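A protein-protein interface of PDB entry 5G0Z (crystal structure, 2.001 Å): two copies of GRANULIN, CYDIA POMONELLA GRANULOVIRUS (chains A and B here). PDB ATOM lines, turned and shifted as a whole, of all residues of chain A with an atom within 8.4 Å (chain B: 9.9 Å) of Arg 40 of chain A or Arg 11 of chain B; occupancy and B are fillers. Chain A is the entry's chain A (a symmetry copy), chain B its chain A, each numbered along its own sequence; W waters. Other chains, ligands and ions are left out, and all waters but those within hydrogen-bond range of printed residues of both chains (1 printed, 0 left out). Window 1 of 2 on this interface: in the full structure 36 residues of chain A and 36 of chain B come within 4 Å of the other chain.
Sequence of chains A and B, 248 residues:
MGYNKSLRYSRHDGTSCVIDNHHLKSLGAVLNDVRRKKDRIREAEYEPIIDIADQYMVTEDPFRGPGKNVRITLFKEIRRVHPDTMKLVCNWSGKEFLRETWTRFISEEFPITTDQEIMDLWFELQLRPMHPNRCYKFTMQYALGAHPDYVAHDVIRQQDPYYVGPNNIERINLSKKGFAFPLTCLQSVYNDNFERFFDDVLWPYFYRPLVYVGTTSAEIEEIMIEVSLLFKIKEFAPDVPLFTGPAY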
ATOM      1  N   ARG A  11     -11.912  11.781  27.704  1.00  0.00           N
ATOM      2  CA  ARG A  11     -11.917  11.089  26.427  1.00  0.00           C
ATOM      3  C   ARG A  11     -10.777  10.076  26.396  1.00  0.00           C
ATOM      4  O   ARG A  11     -10.164   9.835  25.352  1.00  0.00           O
ATOM      5  CB  ARG A  11     -11.843  12.102  25.287  1.00  0.00           C
ATOM      6  CG  ARG A  11     -12.889  13.228  25.436  1.00  0.00           C
ATOM      7  CD  ARG A  11     -12.446  14.518  24.789  1.00  0.00           C
ATOM      8  NE  ARG A  11     -13.189  15.667  25.303  1.00  0.00           N
ATOM      9  CZ  ARG A  11     -13.129  16.889  24.777  1.00  0.00           C
ATOM     10  NH1 ARG A  11     -12.357  17.118  23.718  1.00  0.00           N
ATOM     11  NH2 ARG A  11     -13.842  17.884  25.300  1.00  0.00           N
ATOM     12  N   ASP A  33     -12.504   5.661  17.587  1.00  0.00           N
ATOM     13  CA  ASP A  33     -11.565   6.100  16.556  1.00  0.00           C
ATOM     14  C   ASP A  33     -12.206   6.046  15.173  1.00  0.00           C
ATOM     15  O   ASP A  33     -12.009   6.950  14.349  1.00  0.00           O
ATOM     16  CB  ASP A  33     -10.309   5.224  16.571  1.00  0.00           C
ATOM     17  CG  ASP A  33      -9.495   5.360  17.854  1.00  0.00           C
ATOM     18  OD1 ASP A  33      -9.696   6.334  18.615  1.00  0.00           O
ATOM     19  OD2 ASP A  33      -8.640   4.480  18.095  1.00  0.00           O
ATOM     20  N   VAL A  34     -12.981   4.993  14.901  1.00  0.00           N
ATOM     21  CA  VAL A  34     -13.669   4.886  13.619  1.00  0.00           C
ATOM     22  C   VAL A  34     -14.722   5.978  13.487  1.00  0.00           C
ATOM     23  O   VAL A  34     -14.831   6.641  12.445  1.00  0.00           O
ATOM     24  CB  VAL A  34     -14.269   3.479  13.454  1.00  0.00           C
ATOM     25  CG1 VAL A  34     -15.200   3.424  12.254  1.00  0.00           C
ATOM     26  CG2 VAL A  34     -13.148   2.448  13.312  1.00  0.00           C
ATOM     27  N   ARG A  35     -15.517   6.183  14.537  1.00  0.00           N
ATOM     28  CA  ARG A  35     -16.553   7.209  14.482  1.00  0.00           C
ATOM     29  C   ARG A  35     -15.959   8.608  14.389  1.00  0.00           C
ATOM     30  O   ARG A  35     -16.539   9.478  13.733  1.00  0.00           O
ATOM     31  CB  ARG A  35     -17.466   7.102  15.703  1.00  0.00           C
ATOM     32  CG  ARG A  35     -18.812   7.790  15.534  1.00  0.00           C
ATOM     33  CD  ARG A  35     -19.031   8.812  16.627  1.00  0.00           C
ATOM     34  NE  ARG A  35     -18.995   8.207  17.958  1.00  0.00           N
ATOM     35  CZ  ARG A  35     -18.668   8.858  19.071  1.00  0.00           C
ATOM     36  NH1 ARG A  35     -18.333  10.144  19.023  1.00  0.00           N
ATOM     37  NH2 ARG A  35     -18.662   8.220  20.237  1.00  0.00           N
ATOM     38  N   ARG A  36     -14.811   8.846  15.028  1.00  0.00           N
ATOM     39  CA  ARG A  36     -14.190  10.164  14.953  1.00  0.00           C
ATOM     40  C   ARG A  36     -13.641  10.430  13.558  1.00  0.00           C
ATOM     41  O   ARG A  36     -13.695  11.567  13.070  1.00  0.00           O
ATOM     42  CB  ARG A  36     -13.107  10.303  16.026  1.00  0.00           C
ATOM     43  CG  ARG A  36     -13.652  10.092  17.428  1.00  0.00           C
ATOM     44  CD  ARG A  36     -13.106  11.064  18.444  1.00  0.00           C
ATOM     45  NE  ARG A  36     -13.873  10.999  19.690  1.00  0.00           N
ATOM     46  CZ  ARG A  36     -13.612  10.171  20.702  1.00  0.00           C
ATOM     47  NH1 ARG A  36     -12.594   9.316  20.643  1.00  0.00           N
ATOM     48  NH2 ARG A  36     -14.376  10.202  21.788  1.00  0.00           N
ATOM     49  N   LYS A  37     -13.128   9.392  12.893  1.00  0.00           N
ATOM     50  CA  LYS A  37     -12.690   9.548  11.513  1.00  0.00           C
ATOM     51  C   LYS A  37     -13.862   9.914  10.614  1.00  0.00           C
ATOM     52  O   LYS A  37     -13.732  10.769   9.727  1.00  0.00           O
ATOM     53  CB  LYS A  37     -12.032   8.257  11.028  1.00  0.00           C
ATOM     54  CG  LYS A  37     -11.495   8.318   9.602  1.00  0.00           C
ATOM     55  CD  LYS A  37     -10.312   9.259   9.488  1.00  0.00           C
ATOM     56  CE  LYS A  37      -9.626   9.131   8.129  1.00  0.00           C
ATOM     57  NZ  LYS A  37      -8.313   9.853   8.079  1.00  0.00           N
ATOM     58  N   LYS A  38     -15.012   9.270  10.821  1.00  0.00           N
ATOM     59  CA  LYS A  38     -16.204   9.625  10.059  1.00  0.00           C
ATOM     60  C   LYS A  38     -16.586  11.080  10.309  1.00  0.00           C
ATOM     61  O   LYS A  38     -16.899  11.821   9.370  1.00  0.00           O
ATOM     62  CB  LYS A  38     -17.347   8.680  10.429  1.00  0.00           C
ATOM     63  CG  LYS A  38     -18.678   8.979   9.755  1.00  0.00           C
ATOM     64  CD  LYS A  38     -19.817   8.209  10.424  1.00  0.00           C
ATOM     65  CE  LYS A  38     -21.170   8.922  10.267  1.00  0.00           C
ATOM     66  NZ  LYS A  38     -22.246   8.315  11.122  1.00  0.00           N
ATOM     67  N   ASP A  39     -16.540  11.516  11.569  1.00  0.00           N
ATOM     68  CA  ASP A  39     -16.861  12.907  11.867  1.00  0.00           C
ATOM     69  C   ASP A  39     -15.840  13.857  11.245  1.00  0.00           C
ATOM     70  O   ASP A  39     -16.218  14.876  10.656  1.00  0.00           O
ATOM     71  CB  ASP A  39     -16.958  13.112  13.381  1.00  0.00           C
ATOM     72  CG  ASP A  39     -18.156  12.395  13.993  1.00  0.00           C
ATOM     73  OD1 ASP A  39     -19.101  12.043  13.248  1.00  0.00           O
ATOM     74  OD2 ASP A  39     -18.157  12.196  15.226  1.00  0.00           O
ATOM     75  N   ARG A  40     -14.543  13.543  11.368  1.00  0.00           N
ATOM     76  CA  ARG A  40     -13.504  14.358  10.736  1.00  0.00           C
ATOM     77  C   ARG A  40     -13.774  14.550   9.249  1.00  0.00           C
ATOM     78  O   ARG A  40     -13.568  15.643   8.706  1.00  0.00           O
ATOM     79  CB  ARG A  40     -12.132  13.704  10.931  1.00  0.00           C
ATOM     80  CG  ARG A  40     -11.486  13.939  12.304  1.00  0.00           C
ATOM     81  CD  ARG A  40     -10.814  15.309  12.397  1.00  0.00           C
ATOM     82  NE  ARG A  40     -11.666  16.311  13.034  1.00  0.00           N
ATOM     83  CZ  ARG A  40     -11.527  17.627  12.877  1.00  0.00           C
ATOM     84  NH1 ARG A  40     -10.571  18.113  12.089  1.00  0.00           N
ATOM     85  NH2 ARG A  40     -12.353  18.465  13.501  1.00  0.00           N
ATOM     86  N   ILE A  41     -14.229  13.492   8.570  1.00  0.00           N
ATOM     87  CA  ILE A  41     -14.557  13.597   7.152  1.00  0.00           C
ATOM     88  C   ILE A  41     -15.740  14.535   6.949  1.00  0.00           C
ATOM     89  O   ILE A  41     -15.767  15.325   5.997  1.00  0.00           O
ATOM     90  CB  ILE A  41     -14.796  12.194   6.560  1.00  0.00           C
ATOM     91  CG1 ILE A  41     -13.480  11.401   6.575  1.00  0.00           C
ATOM     92  CG2 ILE A  41     -15.376  12.288   5.142  1.00  0.00           C
ATOM     93  CD1 ILE A  41     -13.588   9.972   6.079  1.00  0.00           C
ATOM     94  N   ARG A  42     -16.730  14.474   7.842  1.00  0.00           N
ATOM     95  CA  ARG A  42     -17.887  15.363   7.746  1.00  0.00           C
ATOM     96  C   ARG A  42     -17.503  16.809   8.048  1.00  0.00           C
ATOM     97  O   ARG A  42     -18.044  17.743   7.443  1.00  0.00           O
ATOM     98  CB  ARG A  42     -18.988  14.872   8.688  1.00  0.00           C
ATOM     99  CG  ARG A  42     -20.166  15.816   8.845  1.00  0.00           C
ATOM    100  CD  ARG A  42     -21.327  15.130   9.561  1.00  0.00           C
ATOM    101  NE  ARG A  42     -21.824  15.899  10.709  1.00  0.00           N
ATOM    102  CZ  ARG A  42     -22.993  16.543  10.758  1.00  0.00           C
ATOM    103  NH1 ARG A  42     -23.826  16.525   9.721  1.00  0.00           N
ATOM    104  NH2 ARG A  42     -23.340  17.206  11.862  1.00  0.00           N
ATOM    105  N   GLU A  43     -16.564  17.014   8.976  1.00  0.00           N
ATOM    106  CA  GLU A  43     -16.068  18.356   9.261  1.00  0.00           C
ATOM    107  C   GLU A  43     -15.465  19.001   8.015  1.00  0.00           C
ATOM    108  O   GLU A  43     -15.624  20.207   7.791  1.00  0.00           O
ATOM    109  CB  GLU A  43     -15.022  18.283  10.371  1.00  0.00           C
ATOM    110  CG  GLU A  43     -14.482  19.626  10.825  1.00  0.00           C
ATOM    111  CD  GLU A  43     -15.146  20.118  12.095  1.00  0.00           C
ATOM    112  OE1 GLU A  43     -16.231  19.603  12.439  1.00  0.00           O
ATOM    113  OE2 GLU A  43     -14.575  21.021  12.750  1.00  0.00           O
ATOM    114  N   ALA A  44     -14.754  18.217   7.197  1.00  0.00           N
ATOM    115  CA  ALA A  44     -14.155  18.761   5.985  1.00  0.00           C
ATOM    116  C   ALA A  44     -15.188  18.990   4.888  1.00  0.00           C
ATOM    117  O   ALA A  44     -14.998  19.871   4.043  1.00  0.00           O
ATOM    118  CB  ALA A  44     -13.047  17.834   5.487  1.00  0.00           C
ATOM    119  N   GLU A  45     -16.286  18.228   4.886  1.00  0.00           N
ATOM    120  CA  GLU A  45     -17.311  18.408   3.861  1.00  0.00           C
ATOM    121  C   GLU A  45     -18.064  19.720   4.039  1.00  0.00           C
ATOM    122  O   GLU A  45     -18.561  20.283   3.059  1.00  0.00           O
ATOM    123  CB  GLU A  45     -18.296  17.237   3.888  1.00  0.00           C
ATOM    124  CG  GLU A  45     -19.411  17.336   2.845  1.00  0.00           C
ATOM    125  CD  GLU A  45     -20.406  16.192   2.937  1.00  0.00           C
ATOM    126  OE1 GLU A  45     -20.338  15.411   3.914  1.00  0.00           O
ATOM    127  OE2 GLU A  45     -21.258  16.075   2.029  1.00  0.00           O
ATOM    128  N   TYR A  46     -18.169  20.218   5.270  1.00  0.00           N
ATOM    129  CA  TYR A  46     -18.949  21.418   5.546  1.00  0.00           C
ATOM    130  C   TYR A  46     -18.089  22.659   5.737  1.00  0.00           C
ATOM    131  O   TYR A  46     -18.631  23.767   5.766  1.00  0.00           O
ATOM    132  CB  TYR A  46     -19.843  21.199   6.775  1.00  0.00           C
ATOM    133  CG  TYR A  46     -20.736  19.974   6.664  1.00  0.00           C
ATOM    134  CD1 TYR A  46     -21.034  19.406   5.422  1.00  0.00           C
ATOM    135  CD2 TYR A  46     -21.280  19.383   7.797  1.00  0.00           C
ATOM    136  CE1 TYR A  46     -21.848  18.280   5.318  1.00  0.00           C
ATOM    137  CE2 TYR A  46     -22.097  18.264   7.704  1.00  0.00           C
ATOM    138  CZ  TYR A  46     -22.378  17.713   6.464  1.00  0.00           C
ATOM    139  OH  TYR A  46     -23.187  16.594   6.373  1.00  0.00           O
ATOM    140  N   GLU A  47     -16.772  22.504   5.856  1.00  0.00           N
ATOM    141  CA  GLU A  47     -15.872  23.654   5.927  1.00  0.00           C
ATOM    142  C   GLU A  47     -16.186  24.720   4.880  1.00  0.00           C
ATOM    143  O   GLU A  47     -16.312  25.898   5.254  1.00  0.00           O
ATOM    144  CB  GLU A  47     -14.420  23.162   5.841  1.00  0.00           C
ATOM    145  CG  GLU A  47     -13.412  24.089   6.518  1.00  0.00           C
ATOM    146  CD  GLU A  47     -11.955  23.657   6.335  1.00  0.00           C
ATOM    147  OE1 GLU A  47     -11.667  22.840   5.431  1.00  0.00           O
ATOM    148  OE2 GLU A  47     -11.092  24.151   7.097  1.00  0.00           O
ATOM    149  N   SER B   6      -6.506  16.702   3.723  1.00  0.00           N
ATOM    150  CA  SER B   6      -6.194  17.874   4.533  1.00  0.00           C
ATOM    151  C   SER B   6      -7.397  18.812   4.644  1.00  0.00           C
ATOM    152  O   SER B   6      -8.362  18.696   3.887  1.00  0.00           O
ATOM    153  CB  SER B   6      -5.001  18.634   3.938  1.00  0.00           C
ATOM    154  OG  SER B   6      -3.785  17.924   4.128  1.00  0.00           O
ATOM    155  N   LEU B   7      -7.331  19.735   5.601  1.00  0.00           N
ATOM    156  CA  LEU B   7      -8.301  20.812   5.749  1.00  0.00           C
ATOM    157  C   LEU B   7      -7.686  22.122   5.280  1.00  0.00           C
ATOM    158  O   LEU B   7      -6.489  22.207   4.991  1.00  0.00           O
ATOM    159  CB  LEU B   7      -8.762  20.942   7.205  1.00  0.00           C
ATOM    160  CG  LEU B   7      -9.987  20.104   7.554  1.00  0.00           C
ATOM    161  CD1 LEU B   7      -9.777  18.656   7.115  1.00  0.00           C
ATOM    162  CD2 LEU B   7     -10.273  20.181   9.040  1.00  0.00           C
ATOM    163  N   ARG B   8      -8.523  23.152   5.207  1.00  0.00           N
ATOM    164  CA  ARG B   8      -8.058  24.459   4.757  1.00  0.00           C
ATOM    165  C   ARG B   8      -7.657  25.362   5.916  1.00  0.00           C
ATOM    166  O   ARG B   8      -6.652  26.076   5.824  1.00  0.00           O
ATOM    167  CB  ARG B   8      -9.142  25.150   3.920  1.00  0.00           C
ATOM    168  CG  ARG B   8      -9.389  24.505   2.566  1.00  0.00           C
ATOM    169  CD  ARG B   8      -8.219  24.720   1.616  1.00  0.00           C
ATOM    170  NE  ARG B   8      -8.223  23.741   0.534  1.00  0.00           N
ATOM    171  CZ  ARG B   8      -8.720  23.950  -0.681  1.00  0.00           C
ATOM    172  NH1 ARG B   8      -9.263  25.120  -0.997  1.00  0.00           N
ATOM    173  NH2 ARG B   8      -8.671  22.982  -1.587  1.00  0.00           N
ATOM    174  N   TYR B   9      -8.422  25.345   7.005  1.00  0.00           N
ATOM    175  CA  TYR B   9      -8.245  26.295   8.096  1.00  0.00           C
ATOM    176  C   TYR B   9      -7.896  25.607   9.405  1.00  0.00           C
ATOM    177  O   TYR B   9      -7.885  26.260  10.455  1.00  0.00           O
ATOM    178  CB  TYR B   9      -9.517  27.141   8.260  1.00  0.00           C
ATOM    179  CG  TYR B   9      -9.957  27.793   6.971  1.00  0.00           C
ATOM    180  CD1 TYR B   9      -9.022  28.308   6.092  1.00  0.00           C
ATOM    181  CD2 TYR B   9     -11.299  27.864   6.617  1.00  0.00           C
ATOM    182  CE1 TYR B   9      -9.400  28.894   4.908  1.00  0.00           C
ATOM    183  CE2 TYR B   9     -11.689  28.457   5.425  1.00  0.00           C
ATOM    184  CZ  TYR B   9     -10.728  28.972   4.578  1.00  0.00           C
ATOM    185  OH  TYR B   9     -11.062  29.566   3.387  1.00  0.00           O
ATOM    186  N   SER B  10      -7.584  24.316   9.370  1.00  0.00           N
ATOM    187  CA  SER B  10      -7.494  23.509  10.585  1.00  0.00           C
ATOM    188  C   SER B  10      -8.845  23.643  11.275  1.00  0.00           C
ATOM    189  O   SER B  10      -9.879  23.334  10.654  1.00  0.00           O
ATOM    190  CB  SER B  10      -6.274  23.950  11.399  1.00  0.00           C
ATOM    191  OG  SER B  10      -5.097  23.949  10.611  1.00  0.00           O
ATOM    192  N   ARG B  11      -8.904  24.110  12.512  1.00  0.00           N
ATOM    193  CA  ARG B  11     -10.164  24.369  13.187  1.00  0.00           C
ATOM    194  C   ARG B  11     -10.146  25.779  13.769  1.00  0.00           C
ATOM    195  O   ARG B  11     -10.709  26.037  14.836  1.00  0.00           O
ATOM    196  CB  ARG B  11     -10.419  23.294  14.241  1.00  0.00           C
ATOM    197  CG  ARG B  11     -10.249  21.867  13.674  1.00  0.00           C
ATOM    198  CD  ARG B  11      -9.834  20.872  14.730  1.00  0.00           C
ATOM    199  NE  ARG B  11      -9.247  19.670  14.142  1.00  0.00           N
ATOM    200  CZ  ARG B  11      -8.967  18.563  14.830  1.00  0.00           C
ATOM    201  NH1 ARG B  11      -9.224  18.511  16.134  1.00  0.00           N
ATOM    202  NH2 ARG B  11      -8.437  17.506  14.219  1.00  0.00           N
ATOM    203  N   HIS B  12      -9.485  26.696  13.057  1.00  0.00           N
ATOM    204  CA  HIS B  12      -9.340  28.091  13.454  1.00  0.00           C
ATOM    205  C   HIS B  12     -10.118  28.981  12.492  1.00  0.00           C
ATOM    206  O   HIS B  12      -9.603  29.996  12.004  1.00  0.00           O
ATOM    207  CB  HIS B  12      -7.860  28.481  13.455  1.00  0.00           C
ATOM    208  CG  HIS B  12      -7.022  27.665  14.392  1.00  0.00           C
ATOM    209  ND1 HIS B  12      -6.510  26.432  14.049  1.00  0.00           N
ATOM    210  CD2 HIS B  12      -6.615  27.901  15.662  1.00  0.00           C
ATOM    211  CE1 HIS B  12      -5.821  25.946  15.067  1.00  0.00           C
ATOM    212  NE2 HIS B  12      -5.869  26.816  16.058  1.00  0.00           N
ATOM    213  N   ASP B  13     -11.364  28.606  12.226  1.00  0.00           N
ATOM    214  CA  ASP B  13     -12.191  29.325  11.270  1.00  0.00           C
ATOM    215  C   ASP B  13     -12.745  30.599  11.896  1.00  0.00           C
ATOM    216  O   ASP B  13     -13.200  30.595  13.042  1.00  0.00           O
ATOM    217  CB  ASP B  13     -13.353  28.437  10.824  1.00  0.00           C
ATOM    218  CG  ASP B  13     -12.905  27.034  10.444  1.00  0.00           C
ATOM    219  OD1 ASP B  13     -12.183  26.396  11.245  1.00  0.00           O
ATOM    220  OD2 ASP B  13     -13.280  26.567   9.346  1.00  0.00           O
ATOM    221  N   GLY B  14     -12.705  31.691  11.127  1.00  0.00           N
ATOM    222  CA  GLY B  14     -13.277  32.956  11.558  1.00  0.00           C
ATOM    223  C   GLY B  14     -12.309  33.778  12.383  1.00  0.00           C
ATOM    224  O   GLY B  14     -11.119  33.468  12.506  1.00  0.00           O
ATOM    225  N   THR B  15     -12.842  34.840  12.982  1.00  0.00           N
ATOM    226  CA  THR B  15     -12.013  35.819  13.677  1.00  0.00           C
ATOM    227  C   THR B  15     -12.899  36.633  14.617  1.00  0.00           C
ATOM    228  O   THR B  15     -14.074  36.308  14.835  1.00  0.00           O
ATOM    229  CB  THR B  15     -11.261  36.686  12.658  1.00  0.00           C
ATOM    230  OG1 THR B  15     -10.350  37.560  13.333  1.00  0.00           O
ATOM    231  CG2 THR B  15     -12.230  37.514  11.841  1.00  0.00           C
ATOM    232  N   LYS B  25     -17.869  38.339  16.615  1.00  0.00           N
ATOM    233  CA  LYS B  25     -17.235  37.090  16.245  1.00  0.00           C
ATOM    234  C   LYS B  25     -17.944  36.558  15.014  1.00  0.00           C
ATOM    235  O   LYS B  25     -19.132  36.818  14.803  1.00  0.00           O
ATOM    236  CB  LYS B  25     -17.316  36.080  17.390  1.00  0.00           C
ATOM    237  CG  LYS B  25     -16.686  34.736  17.100  1.00  0.00           C
ATOM    238  CD  LYS B  25     -16.568  33.905  18.379  1.00  0.00           C
ATOM    239  CE  LYS B  25     -16.061  32.515  18.080  1.00  0.00           C
ATOM    240  NZ  LYS B  25     -16.001  31.655  19.299  1.00  0.00           N
ATOM    241  N   GLY B  28     -20.100  31.852  11.361  1.00  0.00           N
ATOM    242  CA  GLY B  28     -19.829  30.442  11.145  1.00  0.00           C
ATOM    243  C   GLY B  28     -19.116  29.802  12.321  1.00  0.00           C
ATOM    244  O   GLY B  28     -19.392  28.657  12.677  1.00  0.00           O
ATOM    245  N   ALA B  29     -18.180  30.524  12.933  1.00  0.00           N
ATOM    246  CA  ALA B  29     -17.514  29.997  14.116  1.00  0.00           C
ATOM    247  C   ALA B  29     -18.498  29.823  15.272  1.00  0.00           C
ATOM    248  O   ALA B  29     -18.441  28.824  15.998  1.00  0.00           O
ATOM    249  CB  ALA B  29     -16.346  30.908  14.507  1.00  0.00           C
ATOM    250  N   ASN B  32     -20.448  26.730  14.651  1.00  0.00           N
ATOM    251  CA  ASN B  32     -19.652  25.560  15.012  1.00  0.00           C
ATOM    252  C   ASN B  32     -19.643  25.335  16.521  1.00  0.00           C
ATOM    253  O   ASN B  32     -19.779  24.198  16.978  1.00  0.00           O
ATOM    254  CB  ASN B  32     -18.222  25.709  14.493  1.00  0.00           C
ATOM    255  CG  ASN B  32     -18.073  25.282  13.042  1.00  0.00           C
ATOM    256  OD1 ASN B  32     -18.981  24.687  12.461  1.00  0.00           O
ATOM    257  ND2 ASN B  32     -16.912  25.579  12.452  1.00  0.00           N
ATOM    258  N   ASP B  33     -19.480  26.403  17.312  1.00  0.00           N
ATOM    259  CA  ASP B  33     -19.528  26.270  18.767  1.00  0.00           C
ATOM    260  C   ASP B  33     -20.848  25.652  19.216  1.00  0.00           C
ATOM    261  O   ASP B  33     -20.875  24.807  20.122  1.00  0.00           O
ATOM    262  CB  ASP B  33     -19.352  27.637  19.435  1.00  0.00           C
ATOM    263  CG  ASP B  33     -17.976  28.251  19.194  1.00  0.00           C
ATOM    264  OD1 ASP B  33     -17.038  27.530  18.784  1.00  0.00           O
ATOM    265  OD2 ASP B  33     -17.837  29.472  19.427  1.00  0.00           O
ATOM    266  N   ARG B  35     -22.845  23.696  17.326  1.00  0.00           N
ATOM    267  CA  ARG B  35     -22.867  22.308  16.878  1.00  0.00           C
ATOM    268  C   ARG B  35     -21.929  21.434  17.700  1.00  0.00           C
ATOM    269  O   ARG B  35     -22.234  20.261  17.935  1.00  0.00           O
ATOM    270  CB  ARG B  35     -22.503  22.227  15.396  1.00  0.00           C
ATOM    271  CG  ARG B  35     -22.928  20.932  14.721  1.00  0.00           C
ATOM    272  CD  ARG B  35     -21.740  20.242  14.089  1.00  0.00           C
ATOM    273  NE  ARG B  35     -21.088  21.083  13.086  1.00  0.00           N
ATOM    274  CZ  ARG B  35     -19.807  20.983  12.738  1.00  0.00           C
ATOM    275  NH1 ARG B  35     -19.023  20.081  13.320  1.00  0.00           N
ATOM    276  NH2 ARG B  35     -19.304  21.795  11.815  1.00  0.00           N
ATOM    277  N   ARG B  36     -20.795  21.978  18.147  1.00  0.00           N
ATOM    278  CA  ARG B  36     -19.874  21.189  18.956  1.00  0.00           C
ATOM    279  C   ARG B  36     -20.458  20.910  20.335  1.00  0.00           C
ATOM    280  O   ARG B  36     -20.251  19.826  20.896  1.00  0.00           O
ATOM    281  CB  ARG B  36     -18.514  21.886  19.047  1.00  0.00           C
ATOM    282  CG  ARG B  36     -17.894  22.123  17.680  1.00  0.00           C
ATOM    283  CD  ARG B  36     -16.412  21.845  17.629  1.00  0.00           C
ATOM    284  NE  ARG B  36     -15.937  21.811  16.244  1.00  0.00           N
ATOM    285  CZ  ARG B  36     -15.515  22.873  15.558  1.00  0.00           C
ATOM    286  NH1 ARG B  36     -15.496  24.083  16.110  1.00  0.00           N
ATOM    287  NH2 ARG B  36     -15.102  22.721  14.304  1.00  0.00           N
ATOM    288  N   ASP B  39     -22.728  18.053  19.862  1.00  0.00           N
ATOM    289  CA  ASP B  39     -21.964  16.814  19.776  1.00  0.00           C
ATOM    290  C   ASP B  39     -21.422  16.399  21.142  1.00  0.00           C
ATOM    291  O   ASP B  39     -21.505  15.223  21.512  1.00  0.00           O
ATOM    292  CB  ASP B  39     -20.835  16.963  18.753  1.00  0.00           C
ATOM    293  CG  ASP B  39     -21.352  17.092  17.324  1.00  0.00           C
ATOM    294  OD1 ASP B  39     -22.521  16.720  17.064  1.00  0.00           O
ATOM    295  OD2 ASP B  39     -20.580  17.555  16.458  1.00  0.00           O
HETATM  296  O   HOH W   1     -14.560  27.676   7.160  1.00  0.00           O
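OE1 of Glu 47 of chain A lies within hydrogen-bond range of N of Arg 8 of chain B (3.2 Å). The backbone NH (N) of Tyr 9 of chain B is in hydrogen-bond range of the side-chain carboxylate (OE2) of Glu 47 of chain A, at 2.9 Å. The guanidinium group (NH1) of Arg 35 of chain B is in salt-bridge range of the side-chain carboxylate (OE1) of Glu 43 of chain A, at 3.0 Å. The side-chain carboxylate (OE1) of Glu 43 of chain A is in salt-bridge range of the guanidinium group (NH2) of Arg 36 of chain B, 3.8 Å away. The guanidinium group of Arg 40 of chain A lies close to the guanidinium group of Arg 11 of chain B.
OD1 of Asn 32 of chain B is in hydrogen-bond range of NH2 of Arg 35 of chain B (3.0 Å). The guanidinium group (NH2) of Arg 40 of chain A lies within salt-bridge range of the side-chain carboxylate (OE2) of Glu 43 of chain A.
Among the printed residues, pairs that only touch across the chains: Arg 40 of chain A with Leu 7 of chain B (3.7 Å), Ala 44 of chain A with Leu 7 of chain B (3.7 Å), Glu 47 of chain A with Leu 7 of chain B (3.8 Å), Glu 47 of chain A with Ser 10 of chain B (3.8 Å) and Glu 47 of chain A with Asp 13 of chain B (3.8 Å).
Arg 40 of chain A touches just these residues of chain B: Leu 7 (3.7 Å) and Arg 11 (2.9 Å). Glu 43 of chain A touches just these residues of chain B: Arg 35 (3.0 Å) and Arg 36 (2.4 Å). Of chain A, only Glu 47 comes within 4 Å of Ser 10 of chain B. Printed residues of chain B within 4 Å of Glu 47 of chain A: Leu 7, Arg 8, Tyr 9, Ser 10 and Asp 13. Printed residues of chain A within 4 Å of Asp 13 of chain B: Glu 47. Thr 15 of chain B touches none of the printed residues of chain A. Lys 25 of chain B touches none of the printed residues of chain A. The nearest printed residue of chain B that does not touch Glu 47 of chain A is Ser 6 of chain B (5.5 Å).
Hydrophobic or aromatic side chains of chain B that line the printed part of chain A: Leu 7 and Tyr 9. Hydrophobic or aromatic side chains of chain A that line the printed part of chain B: Ala 44.
5 positions are printed for both chains. Of the 10 pairs that touch across the chains among the printed residues, none has its exchanged pair printed and touching as well.
Water W1 lies within hydrogen-bond range of OD2 of Asp 13 of chain B (2.8 Å) and O of Glu 47 of chain A (3.1 Å).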
